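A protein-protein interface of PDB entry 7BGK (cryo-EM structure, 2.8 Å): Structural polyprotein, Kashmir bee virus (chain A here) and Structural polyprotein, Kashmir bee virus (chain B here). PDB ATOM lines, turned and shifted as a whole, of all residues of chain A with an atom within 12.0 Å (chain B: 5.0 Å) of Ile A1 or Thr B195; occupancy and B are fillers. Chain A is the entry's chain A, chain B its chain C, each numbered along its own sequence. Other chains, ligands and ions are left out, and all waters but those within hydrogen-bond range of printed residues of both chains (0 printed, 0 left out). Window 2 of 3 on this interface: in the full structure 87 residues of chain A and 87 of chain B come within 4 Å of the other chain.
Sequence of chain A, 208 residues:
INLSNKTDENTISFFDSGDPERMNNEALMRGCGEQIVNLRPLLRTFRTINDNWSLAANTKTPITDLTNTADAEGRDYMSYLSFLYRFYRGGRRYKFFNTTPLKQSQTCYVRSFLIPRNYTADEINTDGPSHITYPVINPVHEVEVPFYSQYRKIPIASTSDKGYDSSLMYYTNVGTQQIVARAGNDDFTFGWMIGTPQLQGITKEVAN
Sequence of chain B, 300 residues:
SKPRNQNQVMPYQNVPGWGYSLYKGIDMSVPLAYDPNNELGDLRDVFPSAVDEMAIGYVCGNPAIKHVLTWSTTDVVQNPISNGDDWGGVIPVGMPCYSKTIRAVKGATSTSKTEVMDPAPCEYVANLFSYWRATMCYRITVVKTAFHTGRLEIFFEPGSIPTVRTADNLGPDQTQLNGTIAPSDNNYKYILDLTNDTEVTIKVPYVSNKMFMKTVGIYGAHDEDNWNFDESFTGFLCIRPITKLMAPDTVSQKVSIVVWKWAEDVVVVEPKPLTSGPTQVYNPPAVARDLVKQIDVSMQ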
ATOM      1  N   ILE A   1     -30.395 -13.397 -18.011  1.00  0.00           N
ATOM      2  CA  ILE A   1     -29.765 -13.880 -19.265  1.00  0.00           C
ATOM      3  C   ILE A   1     -28.574 -14.757 -18.926  1.00  0.00           C
ATOM      4  O   ILE A   1     -27.804 -14.455 -18.018  1.00  0.00           O
ATOM      5  CB  ILE A   1     -29.346 -12.709 -20.166  1.00  0.00           C
ATOM      6  CG1 ILE A   1     -30.552 -11.840 -20.516  1.00  0.00           C
ATOM      7  CG2 ILE A   1     -28.704 -13.221 -21.437  1.00  0.00           C
ATOM      8  CD1 ILE A   1     -30.187 -10.490 -21.065  1.00  0.00           C
ATOM      9  N   ASN A   2     -28.434 -15.852 -19.665  1.00  0.00           N
ATOM     10  CA  ASN A   2     -27.329 -16.779 -19.482  1.00  0.00           C
ATOM     11  C   ASN A   2     -26.135 -16.329 -20.309  1.00  0.00           C
ATOM     12  O   ASN A   2     -26.266 -16.060 -21.506  1.00  0.00           O
ATOM     13  CB  ASN A   2     -27.741 -18.193 -19.885  1.00  0.00           C
ATOM     14  CG  ASN A   2     -27.030 -19.258 -19.085  1.00  0.00           C
ATOM     15  OD1 ASN A   2     -25.816 -19.203 -18.885  1.00  0.00           O
ATOM     16  ND2 ASN A   2     -27.787 -20.237 -18.617  1.00  0.00           N
ATOM     17  N   LEU A   3     -24.975 -16.246 -19.666  1.00  0.00           N
ATOM     18  CA  LEU A   3     -23.725 -16.017 -20.378  1.00  0.00           C
ATOM     19  C   LEU A   3     -23.446 -17.219 -21.266  1.00  0.00           C
ATOM     20  O   LEU A   3     -23.126 -18.305 -20.775  1.00  0.00           O
ATOM     21  CB  LEU A   3     -22.585 -15.781 -19.396  1.00  0.00           C
ATOM     22  CG  LEU A   3     -22.412 -14.372 -18.835  1.00  0.00           C
ATOM     23  CD1 LEU A   3     -22.036 -13.407 -19.924  1.00  0.00           C
ATOM     24  CD2 LEU A   3     -23.673 -13.914 -18.151  1.00  0.00           C
ATOM     25  N   SER A   4     -23.577 -17.030 -22.572  1.00  0.00           N
ATOM     26  CA  SER A   4     -23.485 -18.129 -23.515  1.00  0.00           C
ATOM     27  C   SER A   4     -23.244 -17.557 -24.900  1.00  0.00           C
ATOM     28  O   SER A   4     -23.732 -16.476 -25.231  1.00  0.00           O
ATOM     29  CB  SER A   4     -24.761 -18.975 -23.504  1.00  0.00           C
ATOM     30  OG  SER A   4     -24.678 -20.064 -24.398  1.00  0.00           O
ATOM     31  N   ASN A   5     -22.465 -18.282 -25.689  1.00  0.00           N
ATOM     32  CA  ASN A   5     -22.362 -18.062 -27.125  1.00  0.00           C
ATOM     33  C   ASN A   5     -22.793 -19.344 -27.818  1.00  0.00           C
ATOM     34  O   ASN A   5     -22.050 -20.330 -27.826  1.00  0.00           O
ATOM     35  CB  ASN A   5     -20.945 -17.668 -27.530  1.00  0.00           C
ATOM     36  CG  ASN A   5     -20.897 -16.995 -28.868  1.00  0.00           C
ATOM     37  OD1 ASN A   5     -21.768 -16.201 -29.207  1.00  0.00           O
ATOM     38  ND2 ASN A   5     -19.887 -17.320 -29.649  1.00  0.00           N
ATOM     39  N   LYS A   6     -23.996 -19.338 -28.382  1.00  0.00           N
ATOM     40  CA  LYS A   6     -24.601 -20.538 -28.927  1.00  0.00           C
ATOM     41  C   LYS A   6     -25.126 -20.265 -30.328  1.00  0.00           C
ATOM     42  O   LYS A   6     -25.111 -19.135 -30.819  1.00  0.00           O
ATOM     43  CB  LYS A   6     -25.732 -21.048 -28.025  1.00  0.00           C
ATOM     44  CG  LYS A   6     -26.877 -20.082 -27.845  1.00  0.00           C
ATOM     45  CD  LYS A   6     -28.038 -20.723 -27.133  1.00  0.00           C
ATOM     46  CE  LYS A   6     -29.224 -19.781 -27.082  1.00  0.00           C
ATOM     47  NZ  LYS A   6     -30.488 -20.446 -26.654  1.00  0.00           N
ATOM     48  N   THR A   7     -25.584 -21.333 -30.971  1.00  0.00           N
ATOM     49  CA  THR A   7     -26.259 -21.276 -32.261  1.00  0.00           C
ATOM     50  C   THR A   7     -27.623 -21.923 -32.097  1.00  0.00           C
ATOM     51  O   THR A   7     -27.718 -23.092 -31.710  1.00  0.00           O
ATOM     52  CB  THR A   7     -25.466 -21.976 -33.365  1.00  0.00           C
ATOM     53  OG1 THR A   7     -25.236 -23.344 -33.011  1.00  0.00           O
ATOM     54  CG2 THR A   7     -24.168 -21.276 -33.612  1.00  0.00           C
ATOM     55  N   ASP A   8     -28.669 -21.164 -32.387  1.00  0.00           N
ATOM     56  CA  ASP A   8     -30.026 -21.676 -32.378  1.00  0.00           C
ATOM     57  C   ASP A   8     -30.473 -22.175 -33.744  1.00  0.00           C
ATOM     58  O   ASP A   8     -31.541 -22.786 -33.844  1.00  0.00           O
ATOM     59  CB  ASP A   8     -30.976 -20.592 -31.878  1.00  0.00           C
ATOM     60  CG  ASP A   8     -30.675 -20.167 -30.461  1.00  0.00           C
ATOM     61  OD1 ASP A   8     -30.706 -21.030 -29.562  1.00  0.00           O
ATOM     62  OD2 ASP A   8     -30.399 -18.970 -30.249  1.00  0.00           O
ATOM     63  N   ASN A  10     -31.459 -20.611 -36.605  1.00  0.00           N
ATOM     64  CA  ASN A  10     -32.682 -19.969 -37.041  1.00  0.00           C
ATOM     65  C   ASN A  10     -32.581 -19.634 -38.518  1.00  0.00           C
ATOM     66  O   ASN A  10     -31.554 -19.144 -38.990  1.00  0.00           O
ATOM     67  CB  ASN A  10     -32.946 -18.706 -36.232  1.00  0.00           C
ATOM     68  CG  ASN A  10     -33.247 -18.998 -34.791  1.00  0.00           C
ATOM     69  OD1 ASN A  10     -34.058 -19.863 -34.473  1.00  0.00           O
ATOM     70  ND2 ASN A  10     -32.587 -18.279 -33.905  1.00  0.00           N
ATOM     71  N   LYS B 144     -17.641 -13.911 -32.074  1.00  0.00           N
ATOM     72  CA  LYS B 144     -17.734 -13.095 -30.881  1.00  0.00           C
ATOM     73  C   LYS B 144     -17.559 -13.991 -29.664  1.00  0.00           C
ATOM     74  O   LYS B 144     -17.110 -15.135 -29.772  1.00  0.00           O
ATOM     75  CB  LYS B 144     -19.064 -12.339 -30.858  1.00  0.00           C
ATOM     76  CG  LYS B 144     -20.267 -13.226 -30.762  1.00  0.00           C
ATOM     77  CD  LYS B 144     -21.509 -12.447 -30.533  1.00  0.00           C
ATOM     78  CE  LYS B 144     -22.540 -13.293 -29.852  1.00  0.00           C
ATOM     79  NZ  LYS B 144     -22.381 -13.314 -28.382  1.00  0.00           N
ATOM     80  N   ALA B 146     -19.261 -14.622 -25.331  1.00  0.00           N
ATOM     81  CA  ALA B 146     -20.421 -14.477 -24.469  1.00  0.00           C
ATOM     82  C   ALA B 146     -20.571 -13.080 -23.897  1.00  0.00           C
ATOM     83  O   ALA B 146     -21.549 -12.831 -23.185  1.00  0.00           O
ATOM     84  CB  ALA B 146     -20.336 -15.486 -23.331  1.00  0.00           C
ATOM     85  N   HIS B 148     -19.817 -10.047 -25.904  1.00  0.00           N
ATOM     86  CA  HIS B 148     -20.270  -9.120 -26.926  1.00  0.00           C
ATOM     87  C   HIS B 148     -21.782  -9.201 -27.053  1.00  0.00           C
ATOM     88  O   HIS B 148     -22.352 -10.294 -27.100  1.00  0.00           O
ATOM     89  CB  HIS B 148     -19.630  -9.445 -28.268  1.00  0.00           C
ATOM     90  CG  HIS B 148     -18.156  -9.213 -28.315  1.00  0.00           C
ATOM     91  ND1 HIS B 148     -17.242 -10.241 -28.264  1.00  0.00           N
ATOM     92  CD2 HIS B 148     -17.436  -8.074 -28.428  1.00  0.00           C
ATOM     93  CE1 HIS B 148     -16.022  -9.744 -28.336  1.00  0.00           C
ATOM     94  NE2 HIS B 148     -16.113  -8.431 -28.437  1.00  0.00           N
ATOM     95  N   THR B 149     -22.430  -8.044 -27.118  1.00  0.00           N
ATOM     96  CA  THR B 149     -23.853  -7.978 -27.385  1.00  0.00           C
ATOM     97  C   THR B 149     -24.111  -6.888 -28.410  1.00  0.00           C
ATOM     98  O   THR B 149     -23.299  -5.982 -28.605  1.00  0.00           O
ATOM     99  CB  THR B 149     -24.668  -7.717 -26.112  1.00  0.00           C
ATOM    100  OG1 THR B 149     -24.414  -6.392 -25.640  1.00  0.00           O
ATOM    101  CG2 THR B 149     -24.308  -8.702 -25.028  1.00  0.00           C
ATOM    102  N   GLY B 150     -25.244  -6.998 -29.077  1.00  0.00           N
ATOM    103  CA  GLY B 150     -25.639  -6.033 -30.076  1.00  0.00           C
ATOM    104  C   GLY B 150     -26.732  -6.582 -30.953  1.00  0.00           C
ATOM    105  O   GLY B 150     -26.943  -7.789 -31.056  1.00  0.00           O
ATOM    106  N   ASP B 193     -30.363 -10.637 -32.509  1.00  0.00           N
ATOM    107  CA  ASP B 193     -29.788 -10.325 -31.210  1.00  0.00           C
ATOM    108  C   ASP B 193     -28.544 -11.170 -30.990  1.00  0.00           C
ATOM    109  O   ASP B 193     -28.580 -12.394 -31.145  1.00  0.00           O
ATOM    110  CB  ASP B 193     -30.800 -10.582 -30.098  1.00  0.00           C
ATOM    111  CG  ASP B 193     -30.397  -9.958 -28.784  1.00  0.00           C
ATOM    112  OD1 ASP B 193     -29.299  -9.372 -28.712  1.00  0.00           O
ATOM    113  OD2 ASP B 193     -31.174 -10.060 -27.816  1.00  0.00           O
ATOM    114  N   LEU B 194     -27.449 -10.514 -30.623  1.00  0.00           N
ATOM    115  CA  LEU B 194     -26.169 -11.169 -30.415  1.00  0.00           C
ATOM    116  C   LEU B 194     -25.878 -11.421 -28.947  1.00  0.00           C
ATOM    117  O   LEU B 194     -24.742 -11.740 -28.595  1.00  0.00           O
ATOM    118  CB  LEU B 194     -25.054 -10.327 -31.022  1.00  0.00           C
ATOM    119  CG  LEU B 194     -24.811 -10.492 -32.512  1.00  0.00           C
ATOM    120  CD1 LEU B 194     -25.848  -9.768 -33.309  1.00  0.00           C
ATOM    121  CD2 LEU B 194     -23.458  -9.938 -32.807  1.00  0.00           C
ATOM    122  N   THR B 195     -26.878 -11.279 -28.083  1.00  0.00           N
ATOM    123  CA  THR B 195     -26.681 -11.546 -26.667  1.00  0.00           C
ATOM    124  C   THR B 195     -26.085 -12.930 -26.453  1.00  0.00           C
ATOM    125  O   THR B 195     -25.069 -13.083 -25.765  1.00  0.00           O
ATOM    126  CB  THR B 195     -28.002 -11.397 -25.917  1.00  0.00           C
ATOM    127  OG1 THR B 195     -28.619 -10.149 -26.258  1.00  0.00           O
ATOM    128  CG2 THR B 195     -27.776 -11.429 -24.438  1.00  0.00           C
ATOM    129  N   ASN B 196     -26.699 -13.954 -27.043  1.00  0.00           N
ATOM    130  CA  ASN B 196     -26.149 -15.301 -26.974  1.00  0.00           C
ATOM    131  C   ASN B 196     -26.034 -15.955 -28.344  1.00  0.00           C
ATOM    132  O   ASN B 196     -25.104 -16.729 -28.585  1.00  0.00           O
ATOM    133  CB  ASN B 196     -27.001 -16.163 -26.050  1.00  0.00           C
ATOM    134  CG  ASN B 196     -26.952 -15.695 -24.622  1.00  0.00           C
ATOM    135  OD1 ASN B 196     -26.000 -15.042 -24.199  1.00  0.00           O
ATOM    136  ND2 ASN B 196     -27.980 -16.018 -23.868  1.00  0.00           N
ATOM    137  N   ASP B 197     -26.960 -15.656 -29.248  1.00  0.00           N
ATOM    138  CA  ASP B 197     -26.908 -16.237 -30.578  1.00  0.00           C
ATOM    139  C   ASP B 197     -25.877 -15.517 -31.439  1.00  0.00           C
ATOM    140  O   ASP B 197     -25.384 -14.438 -31.106  1.00  0.00           O
ATOM    141  CB  ASP B 197     -28.282 -16.193 -31.238  1.00  0.00           C
ATOM    142  CG  ASP B 197     -28.429 -17.207 -32.351  1.00  0.00           C
ATOM    143  OD1 ASP B 197     -27.467 -17.959 -32.604  1.00  0.00           O
ATOM    144  OD2 ASP B 197     -29.507 -17.252 -32.976  1.00  0.00           O
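The side-chain amino group (NZ) of Lys A6 is in salt-bridge range of the side-chain carboxylate (OD1) of Asp A8 (3.0 Å). The side-chain amino group of Lys B144 lies within hydrogen-bond range of the backbone carbonyl oxygen of His B148, 3.3 Å away. NZ of Lys B144 lies within hydrogen-bond range of O of Leu B194, at 2.8 Å. The side-chain carboxylate (OD1) of Asp B193 is in hydrogen-bond range of the side-chain hydroxyl (OG1) of Thr B195 (2.7 Å).
Thr B195 touches Ile A1 (CG2 to CG2, 3.6 Å). Ile A1 touches Asn B196 (CG2 to ND2, 3.8 Å). Leu A3 touches Ala B146 (CD1 to O, 3.3 Å). Ala B146 touches Ser A4. Thr B195 touches Ser A4 (O to O, 3.7 Å). OD1 of Asp B197 touches CA of Thr A7, 3.5 Å away.
Of the 10 printed residues of chain B, 5 touch a printed residue of chain A. Printed residues of chain B that touch a printed residue of chain A: Lys B144, Ala B146, Thr B195, Asn B196 and Asp B197. Hydrophobic or aromatic side chains of chain B within 4 Å of the printed part of chain A: Ala B146. Of the 9 printed residues of chain A, 9 touch a printed residue of chain B. Among the printed residues, 14 pairs touch across the chains.
The backbone carbonyl oxygen of Asn A2 lies close to the side-chain amide oxygen of Asn B196 (2.9 Å). The backbone carbonyl oxygen (O) of Ser A4 lies close to the side-chain amide oxygen (OD1) of Asn B196 (2.9 Å). NZ of Lys B144 lies within hydrogen-bond range of OD1 of Asn A5 (3.1 Å). The backbone carbonyl oxygen of Asn B196 sits close to the side-chain amide oxygen of Asn A5 (3.4 Å). O of Asn B196 lies within hydrogen-bond range of N of Lys A6, at 2.8 Å. N of Asp A8 is in hydrogen-bond range of OD1 of Asp B197. The side-chain amide nitrogen of Asn A10 sits at hydrogen-bond distance from the side-chain carboxylate of Asp B197 (3.4 Å). O of Lys A6 lies close to OD1 of Asp B197, at 3.2 Å.
Of chain B, only Thr B195 (3.6 Å) and Asn B196 (3.8 Å) come within 4 Å of Ile A1. Of the printed residues of chain B, Asp A8 touches Asp B197. Of the printed residues of chain B, Asn A10 touches Asp B197. Of chain A, only Leu A3 and Ser A4 come within 4 Å of Ala B146. His B148 touches none of the printed residues of chain A. No residue of chain A comes within 4 Å of Thr B149. No residue of chain A comes within 4 Å of Gly B150. No residue of chain A comes within 4 Å of Leu B194. Thr B195 touches just these residues of chain A: Ile A1 and Ser A4. The nearest residue of chain A that does not touch Thr B195 is Asn A2 (5.3 Å).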
